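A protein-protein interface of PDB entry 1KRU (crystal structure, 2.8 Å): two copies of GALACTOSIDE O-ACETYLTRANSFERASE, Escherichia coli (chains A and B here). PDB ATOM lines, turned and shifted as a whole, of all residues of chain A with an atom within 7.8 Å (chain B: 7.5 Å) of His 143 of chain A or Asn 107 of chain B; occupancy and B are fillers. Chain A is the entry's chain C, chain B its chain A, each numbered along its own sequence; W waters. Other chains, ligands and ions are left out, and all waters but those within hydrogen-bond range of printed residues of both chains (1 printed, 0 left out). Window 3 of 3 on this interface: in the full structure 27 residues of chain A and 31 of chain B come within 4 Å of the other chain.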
ATOM      1  N   ASN A  87      16.816 -13.963  31.421  1.00  0.00           N
ATOM      2  CA  ASN A  87      15.978 -15.105  31.749  1.00  0.00           C
ATOM      3  C   ASN A  87      16.640 -16.453  31.921  1.00  0.00           C
ATOM      4  O   ASN A  87      16.322 -17.390  31.182  1.00  0.00           O
ATOM      5  CB  ASN A  87      14.880 -15.239  30.699  1.00  0.00           C
ATOM      6  CG  ASN A  87      14.210 -13.919  30.406  1.00  0.00           C
ATOM      7  OD1 ASN A  87      13.379 -13.447  31.195  1.00  0.00           O
ATOM      8  ND2 ASN A  87      14.569 -13.299  29.271  1.00  0.00           N
ATOM      9  N   ILE A 104      26.570 -18.186  29.780  1.00  0.00           N
ATOM     10  CA  ILE A 104      25.237 -18.638  29.414  1.00  0.00           C
ATOM     11  C   ILE A 104      24.428 -17.647  28.609  1.00  0.00           C
ATOM     12  O   ILE A 104      24.264 -16.502  29.005  1.00  0.00           O
ATOM     13  CB  ILE A 104      24.429 -19.042  30.659  1.00  0.00           C
ATOM     14  CG1 ILE A 104      25.176 -20.176  31.379  1.00  0.00           C
ATOM     15  CG2 ILE A 104      22.993 -19.444  30.255  1.00  0.00           C
ATOM     16  CD1 ILE A 104      24.427 -20.831  32.502  1.00  0.00           C
ATOM     17  N   ALA A 105      23.912 -18.114  27.474  1.00  0.00           N
ATOM     18  CA  ALA A 105      23.114 -17.294  26.573  1.00  0.00           C
ATOM     19  C   ALA A 105      21.746 -16.991  27.169  1.00  0.00           C
ATOM     20  O   ALA A 105      21.376 -17.536  28.204  1.00  0.00           O
ATOM     21  CB  ALA A 105      22.954 -18.014  25.242  1.00  0.00           C
ATOM     22  N   PRO A 106      20.982 -16.085  26.537  1.00  0.00           N
ATOM     23  CA  PRO A 106      19.653 -15.745  27.043  1.00  0.00           C
ATOM     24  C   PRO A 106      18.693 -16.923  26.933  1.00  0.00           C
ATOM     25  O   PRO A 106      18.841 -17.783  26.062  1.00  0.00           O
ATOM     26  CB  PRO A 106      19.208 -14.588  26.152  1.00  0.00           C
ATOM     27  CG  PRO A 106      20.428 -14.104  25.485  1.00  0.00           C
ATOM     28  CD  PRO A 106      21.326 -15.284  25.353  1.00  0.00           C
ATOM     29  N   ASN A 107      17.719 -16.959  27.837  1.00  0.00           N
ATOM     30  CA  ASN A 107      16.688 -17.990  27.828  1.00  0.00           C
ATOM     31  C   ASN A 107      17.188 -19.418  27.882  1.00  0.00           C
ATOM     32  O   ASN A 107      16.927 -20.216  26.981  1.00  0.00           O
ATOM     33  CB  ASN A 107      15.800 -17.796  26.598  1.00  0.00           C
ATOM     34  CG  ASN A 107      15.152 -16.426  26.573  1.00  0.00           C
ATOM     35  OD1 ASN A 107      14.556 -15.993  27.570  1.00  0.00           O
ATOM     36  ND2 ASN A 107      15.279 -15.722  25.450  1.00  0.00           N
ATOM     37  N   VAL A 108      17.916 -19.733  28.946  1.00  0.00           N
ATOM     38  CA  VAL A 108      18.435 -21.074  29.145  1.00  0.00           C
ATOM     39  C   VAL A 108      17.676 -21.645  30.332  1.00  0.00           C
ATOM     40  O   VAL A 108      17.376 -20.929  31.290  1.00  0.00           O
ATOM     41  CB  VAL A 108      19.940 -21.048  29.462  1.00  0.00           C
ATOM     42  CG1 VAL A 108      20.388 -22.424  29.939  1.00  0.00           C
ATOM     43  CG2 VAL A 108      20.726 -20.619  28.224  1.00  0.00           C
ATOM     44  N   THR A 109      17.351 -22.929  30.269  1.00  0.00           N
ATOM     45  CA  THR A 109      16.622 -23.569  31.351  1.00  0.00           C
ATOM     46  C   THR A 109      17.326 -24.813  31.868  1.00  0.00           C
ATOM     47  O   THR A 109      17.552 -25.753  31.120  1.00  0.00           O
ATOM     48  CB  THR A 109      15.207 -23.959  30.899  1.00  0.00           C
ATOM     49  OG1 THR A 109      14.469 -22.771  30.601  1.00  0.00           O
ATOM     50  CG2 THR A 109      14.480 -24.730  31.997  1.00  0.00           C
ATOM     51  N   ILE A 140      27.021 -22.218  26.931  1.00  0.00           N
ATOM     52  CA  ILE A 140      25.690 -22.717  26.615  1.00  0.00           C
ATOM     53  C   ILE A 140      24.928 -21.718  25.736  1.00  0.00           C
ATOM     54  O   ILE A 140      24.801 -20.537  26.076  1.00  0.00           O
ATOM     55  CB  ILE A 140      24.896 -22.983  27.902  1.00  0.00           C
ATOM     56  CG1 ILE A 140      25.684 -23.965  28.781  1.00  0.00           C
ATOM     57  CG2 ILE A 140      23.512 -23.528  27.558  1.00  0.00           C
ATOM     58  CD1 ILE A 140      25.329 -23.926  30.257  1.00  0.00           C
ATOM     59  N   GLY A 141      24.424 -22.204  24.603  1.00  0.00           N
ATOM     60  CA  GLY A 141      23.703 -21.354  23.679  1.00  0.00           C
ATOM     61  C   GLY A 141      22.308 -20.969  24.124  1.00  0.00           C
ATOM     62  O   GLY A 141      21.828 -21.407  25.178  1.00  0.00           O
ATOM     63  N   SER A 142      21.659 -20.152  23.299  1.00  0.00           N
ATOM     64  CA  SER A 142      20.309 -19.649  23.542  1.00  0.00           C
ATOM     65  C   SER A 142      19.217 -20.711  23.449  1.00  0.00           C
ATOM     66  O   SER A 142      19.231 -21.566  22.562  1.00  0.00           O
ATOM     67  CB  SER A 142      19.989 -18.539  22.544  1.00  0.00           C
ATOM     68  OG  SER A 142      20.821 -17.416  22.733  1.00  0.00           O
ATOM     69  N   HIS A 143      18.253 -20.628  24.360  1.00  0.00           N
ATOM     70  CA  HIS A 143      17.134 -21.563  24.389  1.00  0.00           C
ATOM     71  C   HIS A 143      17.562 -23.009  24.611  1.00  0.00           C
ATOM     72  O   HIS A 143      17.009 -23.927  24.004  1.00  0.00           O
ATOM     73  CB  HIS A 143      16.339 -21.493  23.086  1.00  0.00           C
ATOM     74  CG  HIS A 143      15.628 -20.197  22.867  1.00  0.00           C
ATOM     75  ND1 HIS A 143      14.439 -20.112  22.176  1.00  0.00           N
ATOM     76  CD2 HIS A 143      15.961 -18.927  23.200  1.00  0.00           C
ATOM     77  CE1 HIS A 143      14.070 -18.842  22.092  1.00  0.00           C
ATOM     78  NE2 HIS A 143      14.975 -18.103  22.705  1.00  0.00           N
ATOM     79  N   VAL A 144      18.543 -23.226  25.470  1.00  0.00           N
ATOM     80  CA  VAL A 144      18.988 -24.575  25.750  1.00  0.00           C
ATOM     81  C   VAL A 144      18.261 -25.072  26.990  1.00  0.00           C
ATOM     82  O   VAL A 144      17.898 -24.285  27.855  1.00  0.00           O
ATOM     83  CB  VAL A 144      20.509 -24.622  26.023  1.00  0.00           C
ATOM     84  CG1 VAL A 144      20.883 -25.924  26.706  1.00  0.00           C
ATOM     85  CG2 VAL A 144      21.271 -24.473  24.718  1.00  0.00           C
ATOM     86  N   VAL A 145      18.041 -26.381  27.065  1.00  0.00           N
ATOM     87  CA  VAL A 145      17.409 -26.983  28.230  1.00  0.00           C
ATOM     88  C   VAL A 145      18.259 -28.168  28.707  1.00  0.00           C
ATOM     89  O   VAL A 145      18.441 -29.140  27.985  1.00  0.00           O
ATOM     90  CB  VAL A 145      16.002 -27.505  27.925  1.00  0.00           C
ATOM     91  CG1 VAL A 145      15.470 -28.223  29.149  1.00  0.00           C
ATOM     92  CG2 VAL A 145      15.073 -26.370  27.553  1.00  0.00           C
ATOM     93  N   ILE A 146      18.787 -28.072  29.920  1.00  0.00           N
ATOM     94  CA  ILE A 146      19.595 -29.140  30.480  1.00  0.00           C
ATOM     95  C   ILE A 146      18.744 -29.932  31.463  1.00  0.00           C
ATOM     96  O   ILE A 146      18.286 -29.403  32.473  1.00  0.00           O
ATOM     97  CB  ILE A 146      20.823 -28.580  31.196  1.00  0.00           C
ATOM     98  CG1 ILE A 146      21.764 -27.956  30.172  1.00  0.00           C
ATOM     99  CG2 ILE A 146      21.545 -29.689  31.928  1.00  0.00           C
ATOM    100  CD1 ILE A 146      22.444 -26.739  30.675  1.00  0.00           C
ATOM    101  N   ILE A 158      27.589 -25.874  23.836  1.00  0.00           N
ATOM    102  CA  ILE A 158      26.250 -26.394  23.596  1.00  0.00           C
ATOM    103  C   ILE A 158      25.514 -25.472  22.625  1.00  0.00           C
ATOM    104  O   ILE A 158      25.108 -24.364  22.991  1.00  0.00           O
ATOM    105  CB  ILE A 158      25.439 -26.484  24.923  1.00  0.00           C
ATOM    106  CG1 ILE A 158      26.268 -27.210  25.994  1.00  0.00           C
ATOM    107  CG2 ILE A 158      24.088 -27.170  24.678  1.00  0.00           C
ATOM    108  CD1 ILE A 158      26.586 -28.668  25.685  1.00  0.00           C
ATOM    109  N   GLY A 159      25.349 -25.935  21.387  1.00  0.00           N
ATOM    110  CA  GLY A 159      24.658 -25.152  20.384  1.00  0.00           C
ATOM    111  C   GLY A 159      23.348 -24.603  20.911  1.00  0.00           C
ATOM    112  O   GLY A 159      22.799 -25.104  21.895  1.00  0.00           O
ATOM    113  N   ALA A 160      22.828 -23.571  20.260  1.00  0.00           N
ATOM    114  CA  ALA A 160      21.580 -22.975  20.703  1.00  0.00           C
ATOM    115  C   ALA A 160      20.404 -23.888  20.419  1.00  0.00           C
ATOM    116  O   ALA A 160      20.411 -24.647  19.453  1.00  0.00           O
ATOM    117  CB  ALA A 160      21.376 -21.627  20.031  1.00  0.00           C
ATOM    118  N   GLY A 161      19.406 -23.823  21.294  1.00  0.00           N
ATOM    119  CA  GLY A 161      18.203 -24.616  21.127  1.00  0.00           C
ATOM    120  C   GLY A 161      18.288 -26.117  21.340  1.00  0.00           C
ATOM    121  O   GLY A 161      17.344 -26.829  20.997  1.00  0.00           O
ATOM    122  N   SER A 162      19.375 -26.621  21.914  1.00  0.00           N
ATOM    123  CA  SER A 162      19.455 -28.060  22.107  1.00  0.00           C
ATOM    124  C   SER A 162      18.821 -28.477  23.419  1.00  0.00           C
ATOM    125  O   SER A 162      18.706 -27.681  24.352  1.00  0.00           O
ATOM    126  CB  SER A 162      20.908 -28.565  22.034  1.00  0.00           C
ATOM    127  OG  SER A 162      21.850 -27.529  22.177  1.00  0.00           O
ATOM    128  N   ILE A 163      18.396 -29.736  23.463  1.00  0.00           N
ATOM    129  CA  ILE A 163      17.772 -30.338  24.640  1.00  0.00           C
ATOM    130  C   ILE A 163      18.701 -31.443  25.127  1.00  0.00           C
ATOM    131  O   ILE A 163      18.689 -32.559  24.608  1.00  0.00           O
ATOM    132  CB  ILE A 163      16.392 -30.952  24.295  1.00  0.00           C
ATOM    133  CG1 ILE A 163      15.449 -29.863  23.782  1.00  0.00           C
ATOM    134  CG2 ILE A 163      15.810 -31.652  25.502  1.00  0.00           C
ATOM    135  CD1 ILE A 163      15.443 -28.593  24.626  1.00  0.00           C
ATOM    136  N   VAL A 177      18.235 -31.786  18.974  1.00  0.00           N
ATOM    137  CA  VAL A 177      17.081 -32.157  19.776  1.00  0.00           C
ATOM    138  C   VAL A 177      16.791 -33.621  19.448  1.00  0.00           C
ATOM    139  O   VAL A 177      16.151 -33.927  18.443  1.00  0.00           O
ATOM    140  CB  VAL A 177      15.845 -31.271  19.430  1.00  0.00           C
ATOM    141  CG1 VAL A 177      14.732 -31.470  20.457  1.00  0.00           C
ATOM    142  CG2 VAL A 177      16.248 -29.814  19.382  1.00  0.00           C
ATOM    143  N   ASN B  85       5.604  -9.828  19.782  1.00  0.00           N
ATOM    144  CA  ASN B  85       4.852 -10.355  20.917  1.00  0.00           C
ATOM    145  C   ASN B  85       5.751 -10.493  22.151  1.00  0.00           C
ATOM    146  O   ASN B  85       6.917 -10.106  22.118  1.00  0.00           O
ATOM    147  CB  ASN B  85       4.235 -11.703  20.559  1.00  0.00           C
ATOM    148  CG  ASN B  85       2.738 -11.735  20.776  1.00  0.00           C
ATOM    149  OD1 ASN B  85       2.232 -11.268  21.800  1.00  0.00           O
ATOM    150  ND2 ASN B  85       2.019 -12.286  19.806  1.00  0.00           N
ATOM    151  N   PHE B  86       5.208 -11.055  23.226  1.00  0.00           N
ATOM    152  CA  PHE B  86       5.953 -11.220  24.476  1.00  0.00           C
ATOM    153  C   PHE B  86       7.397 -11.694  24.392  1.00  0.00           C
ATOM    154  O   PHE B  86       7.767 -12.492  23.532  1.00  0.00           O
ATOM    155  CB  PHE B  86       5.229 -12.189  25.411  1.00  0.00           C
ATOM    156  CG  PHE B  86       3.823 -11.815  25.707  1.00  0.00           C
ATOM    157  CD1 PHE B  86       2.778 -12.548  25.167  1.00  0.00           C
ATOM    158  CD2 PHE B  86       3.539 -10.769  26.565  1.00  0.00           C
ATOM    159  CE1 PHE B  86       1.474 -12.249  25.482  1.00  0.00           C
ATOM    160  CE2 PHE B  86       2.242 -10.467  26.882  1.00  0.00           C
ATOM    161  CZ  PHE B  86       1.204 -11.210  26.340  1.00  0.00           C
ATOM    162  N   ASN B  87       8.201 -11.189  25.316  1.00  0.00           N
ATOM    163  CA  ASN B  87       9.593 -11.587  25.446  1.00  0.00           C
ATOM    164  C   ASN B  87      10.497 -11.658  24.228  1.00  0.00           C
ATOM    165  O   ASN B  87      11.180 -12.664  24.020  1.00  0.00           O
ATOM    166  CB  ASN B  87       9.647 -12.931  26.167  1.00  0.00           C
ATOM    167  CG  ASN B  87       8.815 -12.937  27.429  1.00  0.00           C
ATOM    168  OD1 ASN B  87       9.028 -12.115  28.332  1.00  0.00           O
ATOM    169  ND2 ASN B  87       7.848 -13.855  27.501  1.00  0.00           N
ATOM    170  N   LEU B  88      10.530 -10.607  23.427  1.00  0.00           N
ATOM    171  CA  LEU B  88      11.422 -10.621  22.292  1.00  0.00           C
ATOM    172  C   LEU B  88      12.784 -10.219  22.851  1.00  0.00           C
ATOM    173  O   LEU B  88      12.908  -9.204  23.551  1.00  0.00           O
ATOM    174  CB  LEU B  88      10.954  -9.632  21.225  1.00  0.00           C
ATOM    175  CG  LEU B  88      12.030  -9.190  20.229  1.00  0.00           C
ATOM    176  CD1 LEU B  88      12.163 -10.208  19.117  1.00  0.00           C
ATOM    177  CD2 LEU B  88      11.664  -7.830  19.669  1.00  0.00           C
ATOM    178  N   THR B  89      13.800 -11.030  22.565  1.00  0.00           N
ATOM    179  CA  THR B  89      15.157 -10.771  23.038  1.00  0.00           C
ATOM    180  C   THR B  89      16.085 -10.493  21.873  1.00  0.00           C
ATOM    181  O   THR B  89      16.197 -11.311  20.964  1.00  0.00           O
ATOM    182  CB  THR B  89      15.741 -11.980  23.786  1.00  0.00           C
ATOM    183  OG1 THR B  89      14.813 -12.436  24.775  1.00  0.00           O
ATOM    184  CG2 THR B  89      17.046 -11.608  24.455  1.00  0.00           C
ATOM    185  N   ILE B 104       6.527 -10.833  14.740  1.00  0.00           N
ATOM    186  CA  ILE B 104       7.283 -11.699  15.641  1.00  0.00           C
ATOM    187  C   ILE B 104       6.464 -12.335  16.764  1.00  0.00           C
ATOM    188  O   ILE B 104       5.918 -11.638  17.620  1.00  0.00           O
ATOM    189  CB  ILE B 104       8.469 -10.935  16.255  1.00  0.00           C
ATOM    190  CG1 ILE B 104       9.399 -10.458  15.133  1.00  0.00           C
ATOM    191  CG2 ILE B 104       9.194 -11.824  17.245  1.00  0.00           C
ATOM    192  CD1 ILE B 104      10.760 -10.008  15.575  1.00  0.00           C
ATOM    193  N   ALA B 105       6.407 -13.668  16.747  1.00  0.00           N
ATOM    194  CA  ALA B 105       5.679 -14.453  17.735  1.00  0.00           C
ATOM    195  C   ALA B 105       6.376 -14.368  19.095  1.00  0.00           C
ATOM    196  O   ALA B 105       7.520 -13.932  19.184  1.00  0.00           O
ATOM    197  CB  ALA B 105       5.604 -15.891  17.280  1.00  0.00           C
ATOM    198  N   PRO B 106       5.704 -14.799  20.175  1.00  0.00           N
ATOM    199  CA  PRO B 106       6.321 -14.735  21.511  1.00  0.00           C
ATOM    200  C   PRO B 106       7.599 -15.546  21.672  1.00  0.00           C
ATOM    201  O   PRO B 106       7.788 -16.566  21.005  1.00  0.00           O
ATOM    202  CB  PRO B 106       5.237 -15.257  22.460  1.00  0.00           C
ATOM    203  CG  PRO B 106       3.995 -15.276  21.682  1.00  0.00           C
ATOM    204  CD  PRO B 106       4.351 -15.371  20.224  1.00  0.00           C
ATOM    205  N   ASN B 107       8.471 -15.073  22.561  1.00  0.00           N
ATOM    206  CA  ASN B 107       9.715 -15.762  22.883  1.00  0.00           C
ATOM    207  C   ASN B 107      10.656 -16.058  21.741  1.00  0.00           C
ATOM    208  O   ASN B 107      10.975 -17.214  21.468  1.00  0.00           O
ATOM    209  CB  ASN B 107       9.385 -17.058  23.617  1.00  0.00           C
ATOM    210  CG  ASN B 107       8.489 -16.819  24.811  1.00  0.00           C
ATOM    211  OD1 ASN B 107       8.896 -16.186  25.795  1.00  0.00           O
ATOM    212  ND2 ASN B 107       7.251 -17.296  24.725  1.00  0.00           N
ATOM    213  N   VAL B 108      11.106 -15.000  21.082  1.00  0.00           N
ATOM    214  CA  VAL B 108      12.029 -15.119  19.972  1.00  0.00           C
ATOM    215  C   VAL B 108      13.342 -14.495  20.397  1.00  0.00           C
ATOM    216  O   VAL B 108      13.358 -13.513  21.138  1.00  0.00           O
ATOM    217  CB  VAL B 108      11.490 -14.392  18.737  1.00  0.00           C
ATOM    218  CG1 VAL B 108      12.584 -14.251  17.692  1.00  0.00           C
ATOM    219  CG2 VAL B 108      10.321 -15.159  18.166  1.00  0.00           C
ATOM    220  N   THR B 109      14.448 -15.079  19.944  1.00  0.00           N
ATOM    221  CA  THR B 109      15.769 -14.560  20.283  1.00  0.00           C
ATOM    222  C   THR B 109      16.578 -14.281  19.039  1.00  0.00           C
ATOM    223  O   THR B 109      16.746 -15.147  18.190  1.00  0.00           O
ATOM    224  CB  THR B 109      16.592 -15.534  21.137  1.00  0.00           C
ATOM    225  OG1 THR B 109      15.889 -15.831  22.349  1.00  0.00           O
ATOM    226  CG2 THR B 109      17.933 -14.906  21.492  1.00  0.00           C
ATOM    227  N   LEU B 110      17.075 -13.055  18.943  1.00  0.00           N
ATOM    228  CA  LEU B 110      17.892 -12.628  17.823  1.00  0.00           C
ATOM    229  C   LEU B 110      19.224 -12.242  18.430  1.00  0.00           C
ATOM    230  O   LEU B 110      19.264 -11.487  19.402  1.00  0.00           O
ATOM    231  CB  LEU B 110      17.272 -11.415  17.144  1.00  0.00           C
ATOM    232  CG  LEU B 110      16.177 -11.656  16.106  1.00  0.00           C
ATOM    233  CD1 LEU B 110      14.887 -12.051  16.784  1.00  0.00           C
ATOM    234  CD2 LEU B 110      15.984 -10.377  15.302  1.00  0.00           C
ATOM    235  N   GLY B 141       8.091 -17.463  13.749  1.00  0.00           N
ATOM    236  CA  GLY B 141       7.303 -18.215  14.713  1.00  0.00           C
ATOM    237  C   GLY B 141       7.828 -18.191  16.137  1.00  0.00           C
ATOM    238  O   GLY B 141       8.873 -17.612  16.430  1.00  0.00           O
ATOM    239  N   SER B 142       7.105 -18.855  17.027  1.00  0.00           N
ATOM    240  CA  SER B 142       7.469 -18.901  18.437  1.00  0.00           C
ATOM    241  C   SER B 142       8.750 -19.658  18.770  1.00  0.00           C
ATOM    242  O   SER B 142       9.098 -20.638  18.116  1.00  0.00           O
ATOM    243  CB  SER B 142       6.317 -19.502  19.236  1.00  0.00           C
ATOM    244  OG  SER B 142       5.538 -18.481  19.810  1.00  0.00           O
ATOM    245  N   HIS B 143       9.444 -19.190  19.800  1.00  0.00           N
ATOM    246  CA  HIS B 143      10.671 -19.825  20.262  1.00  0.00           C
ATOM    247  C   HIS B 143      11.765 -19.991  19.218  1.00  0.00           C
ATOM    248  O   HIS B 143      12.592 -20.888  19.340  1.00  0.00           O
ATOM    249  CB  HIS B 143      10.360 -21.203  20.859  1.00  0.00           C
ATOM    250  CG  HIS B 143       9.611 -21.160  22.157  1.00  0.00           C
ATOM    251  ND1 HIS B 143       9.687 -22.172  23.089  1.00  0.00           N
ATOM    252  CD2 HIS B 143       8.729 -20.259  22.651  1.00  0.00           C
ATOM    253  CE1 HIS B 143       8.882 -21.897  24.101  1.00  0.00           C
ATOM    254  NE2 HIS B 143       8.289 -20.744  23.861  1.00  0.00           N
ATOM    255  N   VAL B 144      11.786 -19.144  18.202  1.00  0.00           N
ATOM    256  CA  VAL B 144      12.809 -19.246  17.181  1.00  0.00           C
ATOM    257  C   VAL B 144      14.068 -18.564  17.689  1.00  0.00           C
ATOM    258  O   VAL B 144      13.985 -17.706  18.555  1.00  0.00           O
ATOM    259  CB  VAL B 144      12.351 -18.553  15.868  1.00  0.00           C
ATOM    260  CG1 VAL B 144      13.554 -18.241  14.986  1.00  0.00           C
ATOM    261  CG2 VAL B 144      11.377 -19.447  15.129  1.00  0.00           C
ATOM    262  N   VAL B 145      15.229 -18.968  17.177  1.00  0.00           N
ATOM    263  CA  VAL B 145      16.495 -18.336  17.543  1.00  0.00           C
ATOM    264  C   VAL B 145      17.196 -17.997  16.244  1.00  0.00           C
ATOM    265  O   VAL B 145      17.325 -18.849  15.379  1.00  0.00           O
ATOM    266  CB  VAL B 145      17.444 -19.266  18.364  1.00  0.00           C
ATOM    267  CG1 VAL B 145      18.799 -18.595  18.544  1.00  0.00           C
ATOM    268  CG2 VAL B 145      16.854 -19.553  19.725  1.00  0.00           C
ATOM    269  N   ILE B 146      17.635 -16.752  16.107  1.00  0.00           N
ATOM    270  CA  ILE B 146      18.332 -16.328  14.901  1.00  0.00           C
ATOM    271  C   ILE B 146      19.755 -16.007  15.293  1.00  0.00           C
ATOM    272  O   ILE B 146      19.995 -15.126  16.100  1.00  0.00           O
ATOM    273  CB  ILE B 146      17.685 -15.075  14.265  1.00  0.00           C
ATOM    274  CG1 ILE B 146      16.337 -15.447  13.634  1.00  0.00           C
ATOM    275  CG2 ILE B 146      18.601 -14.505  13.203  1.00  0.00           C
ATOM    276  CD1 ILE B 146      15.292 -14.335  13.700  1.00  0.00           C
ATOM    277  N   GLY B 161      10.068 -22.596  16.784  1.00  0.00           N
ATOM    278  CA  GLY B 161      11.138 -23.425  17.302  1.00  0.00           C
ATOM    279  C   GLY B 161      12.377 -23.591  16.444  1.00  0.00           C
ATOM    280  O   GLY B 161      13.336 -24.211  16.878  1.00  0.00           O
ATOM    281  N   SER B 162      12.408 -23.045  15.243  1.00  0.00           N
ATOM    282  CA  SER B 162      13.601 -23.248  14.453  1.00  0.00           C
ATOM    283  C   SER B 162      14.810 -22.471  14.952  1.00  0.00           C
ATOM    284  O   SER B 162      14.697 -21.447  15.626  1.00  0.00           O
ATOM    285  CB  SER B 162      13.355 -22.924  12.978  1.00  0.00           C
ATOM    286  OG  SER B 162      12.211 -22.132  12.823  1.00  0.00           O
ATOM    287  N   ILE B 163      15.979 -22.995  14.614  1.00  0.00           N
ATOM    288  CA  ILE B 163      17.245 -22.383  14.960  1.00  0.00           C
ATOM    289  C   ILE B 163      17.821 -22.037  13.596  1.00  0.00           C
ATOM    290  O   ILE B 163      18.152 -22.922  12.812  1.00  0.00           O
ATOM    291  CB  ILE B 163      18.194 -23.380  15.689  1.00  0.00           C
ATOM    292  CG1 ILE B 163      17.525 -23.906  16.960  1.00  0.00           C
ATOM    293  CG2 ILE B 163      19.535 -22.694  16.019  1.00  0.00           C
ATOM    294  CD1 ILE B 163      17.105 -22.819  17.944  1.00  0.00           C
HETATM  295  O   HOH W   1      12.699 -22.083  24.087  1.00  0.00           O
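The side-chain hydroxyl (OG1) of Thr 89 of chain B sits at hydrogen-bond distance from the side-chain amide nitrogen (ND2) of Asn 107 of chain A (3.4 Å). The side-chain amide nitrogen (ND2) of Asn 107 of chain A is in hydrogen-bond range of the side-chain hydroxyl (OG1) of Thr 109 of chain B (3.2 Å). The side-chain hydroxyl of Thr 109 of chain B is in hydrogen-bond range of a ring nitrogen (NE2) of His 143 of chain A, at 2.5 Å. A ring nitrogen (ND1) of His 143 of chain A is in hydrogen-bond range of the backbone carbonyl oxygen of His 143 of chain B (3.5 Å).
N of Asn 107 of chain B lies within hydrogen-bond range of O of Phe 86 of chain B. The backbone NH of Leu 110 of chain B sits at hydrogen-bond distance from the backbone carbonyl oxygen of Thr 89 of chain B (2.8 Å). The backbone carbonyl oxygen (O) of Val 144 of chain B lies within hydrogen-bond range of the backbone NH (N) of Thr 109 of chain B (3.0 Å). O of Ser 162 of chain B lies within hydrogen-bond range of N of Val 145 of chain B (3.0 Å). ND2 of Asn 87 of chain A lies within hydrogen-bond range of OD1 of Asn 107 of chain A, at 3.2 Å. N of His 143 of chain A lies within hydrogen-bond range of O of Pro 106 of chain A, 3.4 Å away.
O of Asn 107 of chain B touches CE1 of His 143 of chain A, at 3.6 Å. His 143 of chain A touches Val 144 of chain B. CG of His 143 of chain A touches CG2 of Val 145 of chain B (3.4 Å). O of Ala 160 of chain A touches CG1 of Ile 163 of chain B, at 3.9 Å. CA of Gly 161 of chain A touches CD1 of Ile 163 of chain B (3.8 Å).
Of the printed residues of chain B, His 143 of chain A touches Asn 107, Thr 109, His 143, Val 144 and Val 145. Asn 107 of chain B touches just one residue of chain A: His 143. Of the printed residues of chain A, Thr 109 of chain B touches Asn 107 and His 143. Of the printed residues of chain A, Ile 163 of chain B touches Ala 160 and Gly 161. Val 177 of chain A touches none of the printed residues of chain B. Ser 162 of chain B touches none of the printed residues of chain A. The nearest residue of chain A that does not touch Asn 107 of chain B is Asn 107 of chain A (5.9 Å). The nearest printed residue of chain A that does not touch Thr 109 of chain B is Ser 142 of chain A (4.02 Å).
Of the 21 printed residues of chain B, 7 touch a printed residue of chain A. Printed residues of chain B that touch a printed residue of chain A: Thr 89, Asn 107, Thr 109, His 143, Val 144, Val 145 and Ile 163. Hydrophobic or aromatic side chains of chain B that line the printed part of chain A: Val 145 and Ile 163. Along chain B the printed residues that touch a printed residue of chain A span positions 89 to 163. Among the printed residues, no Asp or Glu carboxylate lies within 4 Å of a Lys or Arg side-chain nitrogen of the other chain.
Asn 107 of chain A touches Thr 109 of chain B, but with the chains exchanged Thr 109 of chain A does not touch Asn 107 of chain B (9.9 Å). His 143 of chain A touches Asn 107 of chain B, but with the chains exchanged Asn 107 of chain A does not touch His 143 of chain B (8.1 Å). His 143 of chain A touches Val 144 of chain B, but with the chains exchanged Val 144 of chain A does not touch His 143 of chain B (8.9 Å). Gly 161 of chain A touches Ile 163 of chain B, but with the chains exchanged Ile 163 of chain A does not touch Gly 161 of chain B (9.1 Å). Of the 9 pairs that touch across the chains among the printed residues, 1 has its exchanged pair printed and touching as well.
Water W1 lies within hydrogen-bond range of ND1 of His 143 of chain B and ND1 of His 143 of chain A.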
